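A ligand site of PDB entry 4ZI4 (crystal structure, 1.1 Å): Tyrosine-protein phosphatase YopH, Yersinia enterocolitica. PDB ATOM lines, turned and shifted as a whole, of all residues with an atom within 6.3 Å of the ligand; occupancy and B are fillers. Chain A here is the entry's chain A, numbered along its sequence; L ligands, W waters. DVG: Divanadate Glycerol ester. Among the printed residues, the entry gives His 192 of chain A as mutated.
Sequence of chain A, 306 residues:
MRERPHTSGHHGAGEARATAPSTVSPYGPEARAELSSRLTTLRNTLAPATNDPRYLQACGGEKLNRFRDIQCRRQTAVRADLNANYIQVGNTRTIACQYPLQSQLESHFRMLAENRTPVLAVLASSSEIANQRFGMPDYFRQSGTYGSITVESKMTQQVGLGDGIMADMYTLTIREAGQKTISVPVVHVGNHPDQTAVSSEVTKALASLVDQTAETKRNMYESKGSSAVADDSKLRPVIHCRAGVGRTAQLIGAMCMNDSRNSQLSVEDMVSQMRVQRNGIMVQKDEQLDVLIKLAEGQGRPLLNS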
ATOM      1  N   PHE A  67      19.240   5.763  -4.099  1.00  0.00           N
ATOM      2  CA  PHE A  67      20.503   6.014  -3.403  1.00  0.00           C
ATOM      3  C   PHE A  67      20.721   7.523  -3.347  1.00  0.00           C
ATOM      4  O   PHE A  67      20.626   8.218  -4.366  1.00  0.00           O
ATOM      5  CB  PHE A  67      21.678   5.343  -4.129  1.00  0.00           C
ATOM      6  CG  PHE A  67      21.500   3.863  -4.273  1.00  0.00           C
ATOM      7  CD1 PHE A  67      20.975   3.310  -5.425  1.00  0.00           C
ATOM      8  CD2 PHE A  67      21.860   3.009  -3.233  1.00  0.00           C
ATOM      9  CE1 PHE A  67      20.805   1.936  -5.542  1.00  0.00           C
ATOM     10  CE2 PHE A  67      21.701   1.643  -3.344  1.00  0.00           C
ATOM     11  CZ  PHE A  67      21.170   1.104  -4.506  1.00  0.00           C
ATOM     12  N   ILE A  70      23.042   9.206  -5.900  1.00  0.00           N
ATOM     13  CA  ILE A  70      22.903   8.823  -7.306  1.00  0.00           C
ATOM     14  C   ILE A  70      21.659   9.522  -7.836  1.00  0.00           C
ATOM     15  O   ILE A  70      20.525   9.029  -7.680  1.00  0.00           O
ATOM     16  CB  ILE A  70      22.859   7.303  -7.456  1.00  0.00           C
ATOM     17  CG1 ILE A  70      24.104   6.708  -6.805  1.00  0.00           C
ATOM     18  CG2 ILE A  70      22.745   6.928  -8.905  1.00  0.00           C
ATOM     19  CD1 ILE A  70      24.262   5.206  -6.916  1.00  0.00           C
ATOM     20  N   ALA A 124      19.533  -6.261 -12.950  1.00  0.00           N
ATOM     21  CA  ALA A 124      19.501  -6.788 -11.570  1.00  0.00           C
ATOM     22  C   ALA A 124      19.111  -8.253 -11.630  1.00  0.00           C
ATOM     23  O   ALA A 124      18.173  -8.616 -12.339  1.00  0.00           O
ATOM     24  CB  ALA A 124      18.513  -6.019 -10.715  1.00  0.00           C
ATOM     25  N   GLU A 128      19.039 -10.693  -6.453  1.00  0.00           N
ATOM     26  CA  GLU A 128      18.941  -9.325  -5.942  1.00  0.00           C
ATOM     27  C   GLU A 128      17.483  -8.910  -5.767  1.00  0.00           C
ATOM     28  O   GLU A 128      17.097  -8.353  -4.736  1.00  0.00           O
ATOM     29  CB  GLU A 128      19.661  -8.344  -6.861  1.00  0.00           C
ATOM     30  CG  GLU A 128      21.167  -8.442  -6.830  1.00  0.00           C
ATOM     31  CD  GLU A 128      21.800  -7.572  -7.900  1.00  0.00           C
ATOM     32  OE1 GLU A 128      22.425  -6.551  -7.580  1.00  0.00           O
ATOM     33  OE2 GLU A 128      21.645  -7.886  -9.079  1.00  0.00           O
ATOM     34  N   HIS A 192      22.626 -12.656 -13.701  1.00  0.00           N
ATOM     35  CA  HIS A 192      23.739 -11.723 -13.712  1.00  0.00           C
ATOM     36  C   HIS A 192      24.497 -11.855 -12.409  1.00  0.00           C
ATOM     37  O   HIS A 192      23.889 -11.859 -11.341  1.00  0.00           O
ATOM     38  CB  HIS A 192      23.228 -10.294 -13.865  1.00  0.00           C
ATOM     39  CG  HIS A 192      24.324  -9.333 -14.188  1.00  0.00           C
ATOM     40  ND1 HIS A 192      25.368  -9.077 -13.327  1.00  0.00           N
ATOM     41  CD2 HIS A 192      24.548  -8.579 -15.291  1.00  0.00           C
ATOM     42  CE1 HIS A 192      26.194  -8.222 -13.893  1.00  0.00           C
ATOM     43  NE2 HIS A 192      25.725  -7.903 -15.079  1.00  0.00           N
ATOM     44  N   PRO A 193      25.829 -11.969 -12.472  1.00  0.00           N
ATOM     45  CA  PRO A 193      26.581 -12.081 -11.210  1.00  0.00           C
ATOM     46  C   PRO A 193      26.422 -10.827 -10.346  1.00  0.00           C
ATOM     47  O   PRO A 193      26.219  -9.739 -10.882  1.00  0.00           O
ATOM     48  CB  PRO A 193      28.038 -12.238 -11.673  1.00  0.00           C
ATOM     49  CG  PRO A 193      28.069 -11.720 -13.056  1.00  0.00           C
ATOM     50  CD  PRO A 193      26.731 -12.044 -13.642  1.00  0.00           C
ATOM     51  N   ASP A 194      26.528 -10.987  -9.030  1.00  0.00           N
ATOM     52  CA  ASP A 194      26.226  -9.916  -8.094  1.00  0.00           C
ATOM     53  C   ASP A 194      27.426  -9.057  -7.628  1.00  0.00           C
ATOM     54  O   ASP A 194      27.221  -7.938  -7.165  1.00  0.00           O
ATOM     55  CB  ASP A 194      25.513 -10.483  -6.853  1.00  0.00           C
ATOM     56  CG  ASP A 194      24.308 -11.350  -7.204  1.00  0.00           C
ATOM     57  OD1 ASP A 194      23.713 -11.170  -8.291  1.00  0.00           O
ATOM     58  OD2 ASP A 194      23.961 -12.230  -6.386  1.00  0.00           O
ATOM     59  N   THR A 196      30.690  -9.008  -9.497  1.00  0.00           N
ATOM     60  CA  THR A 196      31.697  -8.886 -10.534  1.00  0.00           C
ATOM     61  C   THR A 196      31.044  -8.473 -11.836  1.00  0.00           C
ATOM     62  O   THR A 196      29.813  -8.449 -11.942  1.00  0.00           O
ATOM     63  CB  THR A 196      32.481 -10.196 -10.737  1.00  0.00           C
ATOM     64  OG1 THR A 196      33.497 -10.002 -11.733  1.00  0.00           O
ATOM     65  CG2 THR A 196      31.554 -11.323 -11.161  1.00  0.00           C
ATOM     66  N   CYS A 241      19.646  -1.463 -13.789  1.00  0.00           N
ATOM     67  CA  CYS A 241      20.072  -2.458 -12.823  1.00  0.00           C
ATOM     68  C   CYS A 241      19.414  -2.057 -11.498  1.00  0.00           C
ATOM     69  O   CYS A 241      18.201  -1.897 -11.492  1.00  0.00           O
ATOM     70  CB  CYS A 241      21.617  -2.589 -12.797  1.00  0.00           C
ATOM     71  SG  CYS A 241      22.532  -1.026 -12.787  1.00  0.00           S
ATOM     72  N   ARG A 242      20.144  -1.931 -10.394  1.00  0.00           N
ATOM     73  CA  ARG A 242      19.554  -1.400  -9.158  1.00  0.00           C
ATOM     74  C   ARG A 242      19.623   0.124  -9.159  1.00  0.00           C
ATOM     75  O   ARG A 242      18.607   0.789  -8.996  1.00  0.00           O
ATOM     76  CB  ARG A 242      20.224  -1.973  -7.886  1.00  0.00           C
ATOM     77  CG  ARG A 242      20.359  -3.478  -7.854  1.00  0.00           C
ATOM     78  CD  ARG A 242      20.670  -4.005  -6.455  1.00  0.00           C
ATOM     79  NE  ARG A 242      21.778  -3.310  -5.798  1.00  0.00           N
ATOM     80  CZ  ARG A 242      22.894  -3.872  -5.366  1.00  0.00           C
ATOM     81  NH1 ARG A 242      23.820  -3.125  -4.780  1.00  0.00           N
ATOM     82  NH2 ARG A 242      23.109  -5.177  -5.500  1.00  0.00           N
ATOM     83  N   ALA A 243      20.818   0.682  -9.345  1.00  0.00           N
ATOM     84  CA  ALA A 243      20.990   2.142  -9.370  1.00  0.00           C
ATOM     85  C   ALA A 243      20.958   2.762 -10.773  1.00  0.00           C
ATOM     86  O   ALA A 243      20.790   3.967 -10.915  1.00  0.00           O
ATOM     87  CB  ALA A 243      22.317   2.506  -8.692  1.00  0.00           C
ATOM     88  N   GLY A 244      21.162   1.953 -11.813  1.00  0.00           N
ATOM     89  CA  GLY A 244      21.178   2.477 -13.178  1.00  0.00           C
ATOM     90  C   GLY A 244      22.420   3.272 -13.543  1.00  0.00           C
ATOM     91  O   GLY A 244      22.345   4.151 -14.396  1.00  0.00           O
ATOM     92  N   VAL A 245      23.571   2.907 -12.958  1.00  0.00           N
ATOM     93  CA  VAL A 245      24.835   3.595 -13.275  1.00  0.00           C
ATOM     94  C   VAL A 245      26.030   2.653 -13.538  1.00  0.00           C
ATOM     95  O   VAL A 245      27.073   3.115 -14.001  1.00  0.00           O
ATOM     96  CB  VAL A 245      25.242   4.602 -12.168  1.00  0.00           C
ATOM     97  CG1 VAL A 245      24.223   5.711 -12.089  1.00  0.00           C
ATOM     98  CG2 VAL A 245      25.417   3.919 -10.850  1.00  0.00           C
ATOM     99  N   GLY A 246      25.904   1.367 -13.232  1.00  0.00           N
ATOM    100  CA  GLY A 246      27.041   0.449 -13.326  1.00  0.00           C
ATOM    101  C   GLY A 246      26.850  -0.498 -14.487  1.00  0.00           C
ATOM    102  O   GLY A 246      27.245  -0.205 -15.615  1.00  0.00           O
ATOM    103  N   ARG A 247      26.190  -1.613 -14.214  1.00  0.00           N
ATOM    104  CA  ARG A 247      25.848  -2.575 -15.267  1.00  0.00           C
ATOM    105  C   ARG A 247      25.132  -1.872 -16.428  1.00  0.00           C
ATOM    106  O   ARG A 247      25.359  -2.174 -17.606  1.00  0.00           O
ATOM    107  CB  ARG A 247      24.966  -3.682 -14.711  1.00  0.00           C
ATOM    108  CG  ARG A 247      25.658  -4.516 -13.641  1.00  0.00           C
ATOM    109  CD  ARG A 247      24.684  -5.436 -12.934  1.00  0.00           C
ATOM    110  NE  ARG A 247      25.188  -5.896 -11.650  1.00  0.00           N
ATOM    111  CZ  ARG A 247      24.504  -6.654 -10.809  1.00  0.00           C
ATOM    112  NH1 ARG A 247      23.274  -7.062 -11.130  1.00  0.00           N
ATOM    113  NH2 ARG A 247      25.027  -7.023  -9.649  1.00  0.00           N
ATOM    114  N   THR A 248      24.242  -0.956 -16.068  1.00  0.00           N
ATOM    115  CA  THR A 248      23.471  -0.189 -17.050  1.00  0.00           C
ATOM    116  C   THR A 248      24.380   0.598 -17.992  1.00  0.00           C
ATOM    117  O   THR A 248      24.157   0.597 -19.211  1.00  0.00           O
ATOM    118  CB  THR A 248      22.526   0.763 -16.281  1.00  0.00           C
ATOM    119  OG1 THR A 248      21.502  -0.029 -15.659  1.00  0.00           O
ATOM    120  CG2 THR A 248      21.855   1.774 -17.196  1.00  0.00           C
ATOM    121  N   GLN A 284      30.285   3.096 -13.013  1.00  0.00           N
ATOM    122  CA  GLN A 284      30.534   3.315 -11.597  1.00  0.00           C
ATOM    123  C   GLN A 284      31.884   2.758 -11.172  1.00  0.00           C
ATOM    124  O   GLN A 284      32.561   3.345 -10.328  1.00  0.00           O
ATOM    125  CB  GLN A 284      29.404   2.671 -10.794  1.00  0.00           C
ATOM    126  CG  GLN A 284      29.549   2.838  -9.306  1.00  0.00           C
ATOM    127  CD  GLN A 284      28.285   2.474  -8.551  1.00  0.00           C
ATOM    128  OE1 GLN A 284      27.569   1.533  -8.916  1.00  0.00           O
ATOM    129  NE2 GLN A 284      27.997   3.218  -7.510  1.00  0.00           N
ATOM    130  N   LYS A 285      32.264   1.636 -11.759  1.00  0.00           N
ATOM    131  CA  LYS A 285      33.419   0.863 -11.319  1.00  0.00           C
ATOM    132  C   LYS A 285      34.478   0.744 -12.402  1.00  0.00           C
ATOM    133  O   LYS A 285      34.165   0.629 -13.590  1.00  0.00           O
ATOM    134  CB  LYS A 285      32.964  -0.543 -10.891  1.00  0.00           C
ATOM    135  CG  LYS A 285      31.927  -0.524  -9.790  1.00  0.00           C
ATOM    136  CD  LYS A 285      31.496  -1.909  -9.328  1.00  0.00           C
ATOM    137  CE  LYS A 285      30.491  -1.818  -8.190  1.00  0.00           C
ATOM    138  NZ  LYS A 285      29.978  -3.152  -7.744  1.00  0.00           N
ATOM    139  N   GLN A 288      34.022  -2.027 -14.913  1.00  0.00           N
ATOM    140  CA  GLN A 288      33.106  -1.768 -16.014  1.00  0.00           C
ATOM    141  C   GLN A 288      33.811  -0.977 -17.120  1.00  0.00           C
ATOM    142  O   GLN A 288      33.652  -1.269 -18.307  1.00  0.00           O
ATOM    143  CB  GLN A 288      31.887  -1.023 -15.491  1.00  0.00           C
ATOM    144  CG  GLN A 288      31.082  -1.872 -14.539  1.00  0.00           C
ATOM    145  CD  GLN A 288      30.299  -1.088 -13.515  1.00  0.00           C
ATOM    146  OE1 GLN A 288      30.366   0.149 -13.441  1.00  0.00           O
ATOM    147  NE2 GLN A 288      29.529  -1.799 -12.714  1.00  0.00           N
HETATM  148  O3  DVG L   1      27.009  -2.670  -8.299  1.00  0.00           O
HETATM  149  C3  DVG L   1      26.374  -1.826  -7.352  1.00  0.00           C
HETATM  150  C2  DVG L   1      25.040  -1.398  -7.930  1.00  0.00           C
HETATM  151  O2  DVG L   1      25.321  -0.996  -9.256  1.00  0.00           O
HETATM  152  C1  DVG L   1      24.393  -0.263  -7.149  1.00  0.00           C
HETATM  153  O1  DVG L   1      25.293   0.813  -7.048  1.00  0.00           O
HETATM  154  O01 DVG L   1      27.999  -0.983 -10.392  1.00  0.00           O
HETATM  155  V02 DVG L   1      26.733  -2.099 -10.140  1.00  0.00           V
HETATM  156  O03 DVG L   1      27.383  -3.763 -10.704  1.00  0.00           O
HETATM  157  V06 DVG L   1      24.097  -1.008 -10.834  1.00  0.00           V
HETATM  158  O07 DVG L   1      24.150   0.738 -11.018  1.00  0.00           O
HETATM  159  O08 DVG L   1      22.810  -1.748  -9.803  1.00  0.00           O
HETATM  160  O09 DVG L   1      25.435  -2.046 -11.545  1.00  0.00           O
HETATM  161  O   HOH W   1      26.127  -5.068  -7.331  1.00  0.00           O
HETATM  162  O   HOH W   2      26.136   2.328  -5.250  1.00  0.00           O
HETATM  163  O   HOH W   3      29.336  -4.804 -12.827  1.00  0.00           O
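SG of Cys 241 is bound to V06 of the ligand (2.5 Å).
N of Arg 242 sits close to O08 of the ligand (2.7 Å).
The side-chain amide oxygen of Gln 284 sits at hydrogen-bond distance from an oxygen (O1) of the ligand, at 3.0 Å.
The side-chain sulfur (SG) of Cys 241 lies close to the backbone NH (N) of Gly 244 (3.4 Å).
The side-chain hydroxyl (OG1) of Thr 248 lies within hydrogen-bond range of the backbone NH (N) of Cys 241 (3.0 Å).
The guanidinium group (NH2) of Arg 242 lies within salt-bridge range of the side-chain carboxylate (OE1) of Glu 128 (2.6 Å).
NH2 of Arg 247 is in hydrogen-bond range of O of Asp 194, 3.4 Å away.
O of Pro 193 is in hydrogen-bond range of NH2 of Arg 247 (3.2 Å).
N of Gln 284 is in hydrogen-bond range of OE1 of Gln 288.
The side-chain amide oxygen of Gln 288 lies within hydrogen-bond range of the backbone NH of Lys 285.
The backbone NH of Gln 284 is in hydrogen-bond range of the backbone carbonyl oxygen of Val 245, at 3.4 Å.
N of Ala 243 lies close to O08 of the ligand (3.2 Å).
The backbone NH (N) of Gly 244 sits close to an oxygen (O07) of the ligand, at 3.3 Å.
N of Val 245 lies close to O07 of the ligand.
N of Gly 246 sits close to O07 of the ligand.
O09 of the ligand lies close to N of Arg 247, 2.8 Å away.
The side-chain amino group of Lys 285 sits close to an oxygen (O3) of the ligand (3.1 Å).
An oxygen (O01) of the ligand lies close to the side-chain amide nitrogen of Gln 288.
Hydrophobic or aromatic side chains that line the ligand: Ala 243 and Val 245.
Ten residues have an atom within 4 Å of the ligand: Cys 241, Arg 242, Ala 243, Gly 244, Val 245, Gly 246, Arg 247, Gln 284, Lys 285 and Gln 288.
The nearest printed residue that does not touch the ligand is Phe 67 (4.4 Å).
Water W2 lies within hydrogen-bond range of O1 of the ligand (2.5 Å) and NE2 of Gln 284 (3.1 Å).
Water W1 lies within hydrogen-bond range of the backbone carbonyl oxygen (O) of Asp 194 (3.1 Å) and the guanidinium group (NH2) of Arg 247 (3.2 Å).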
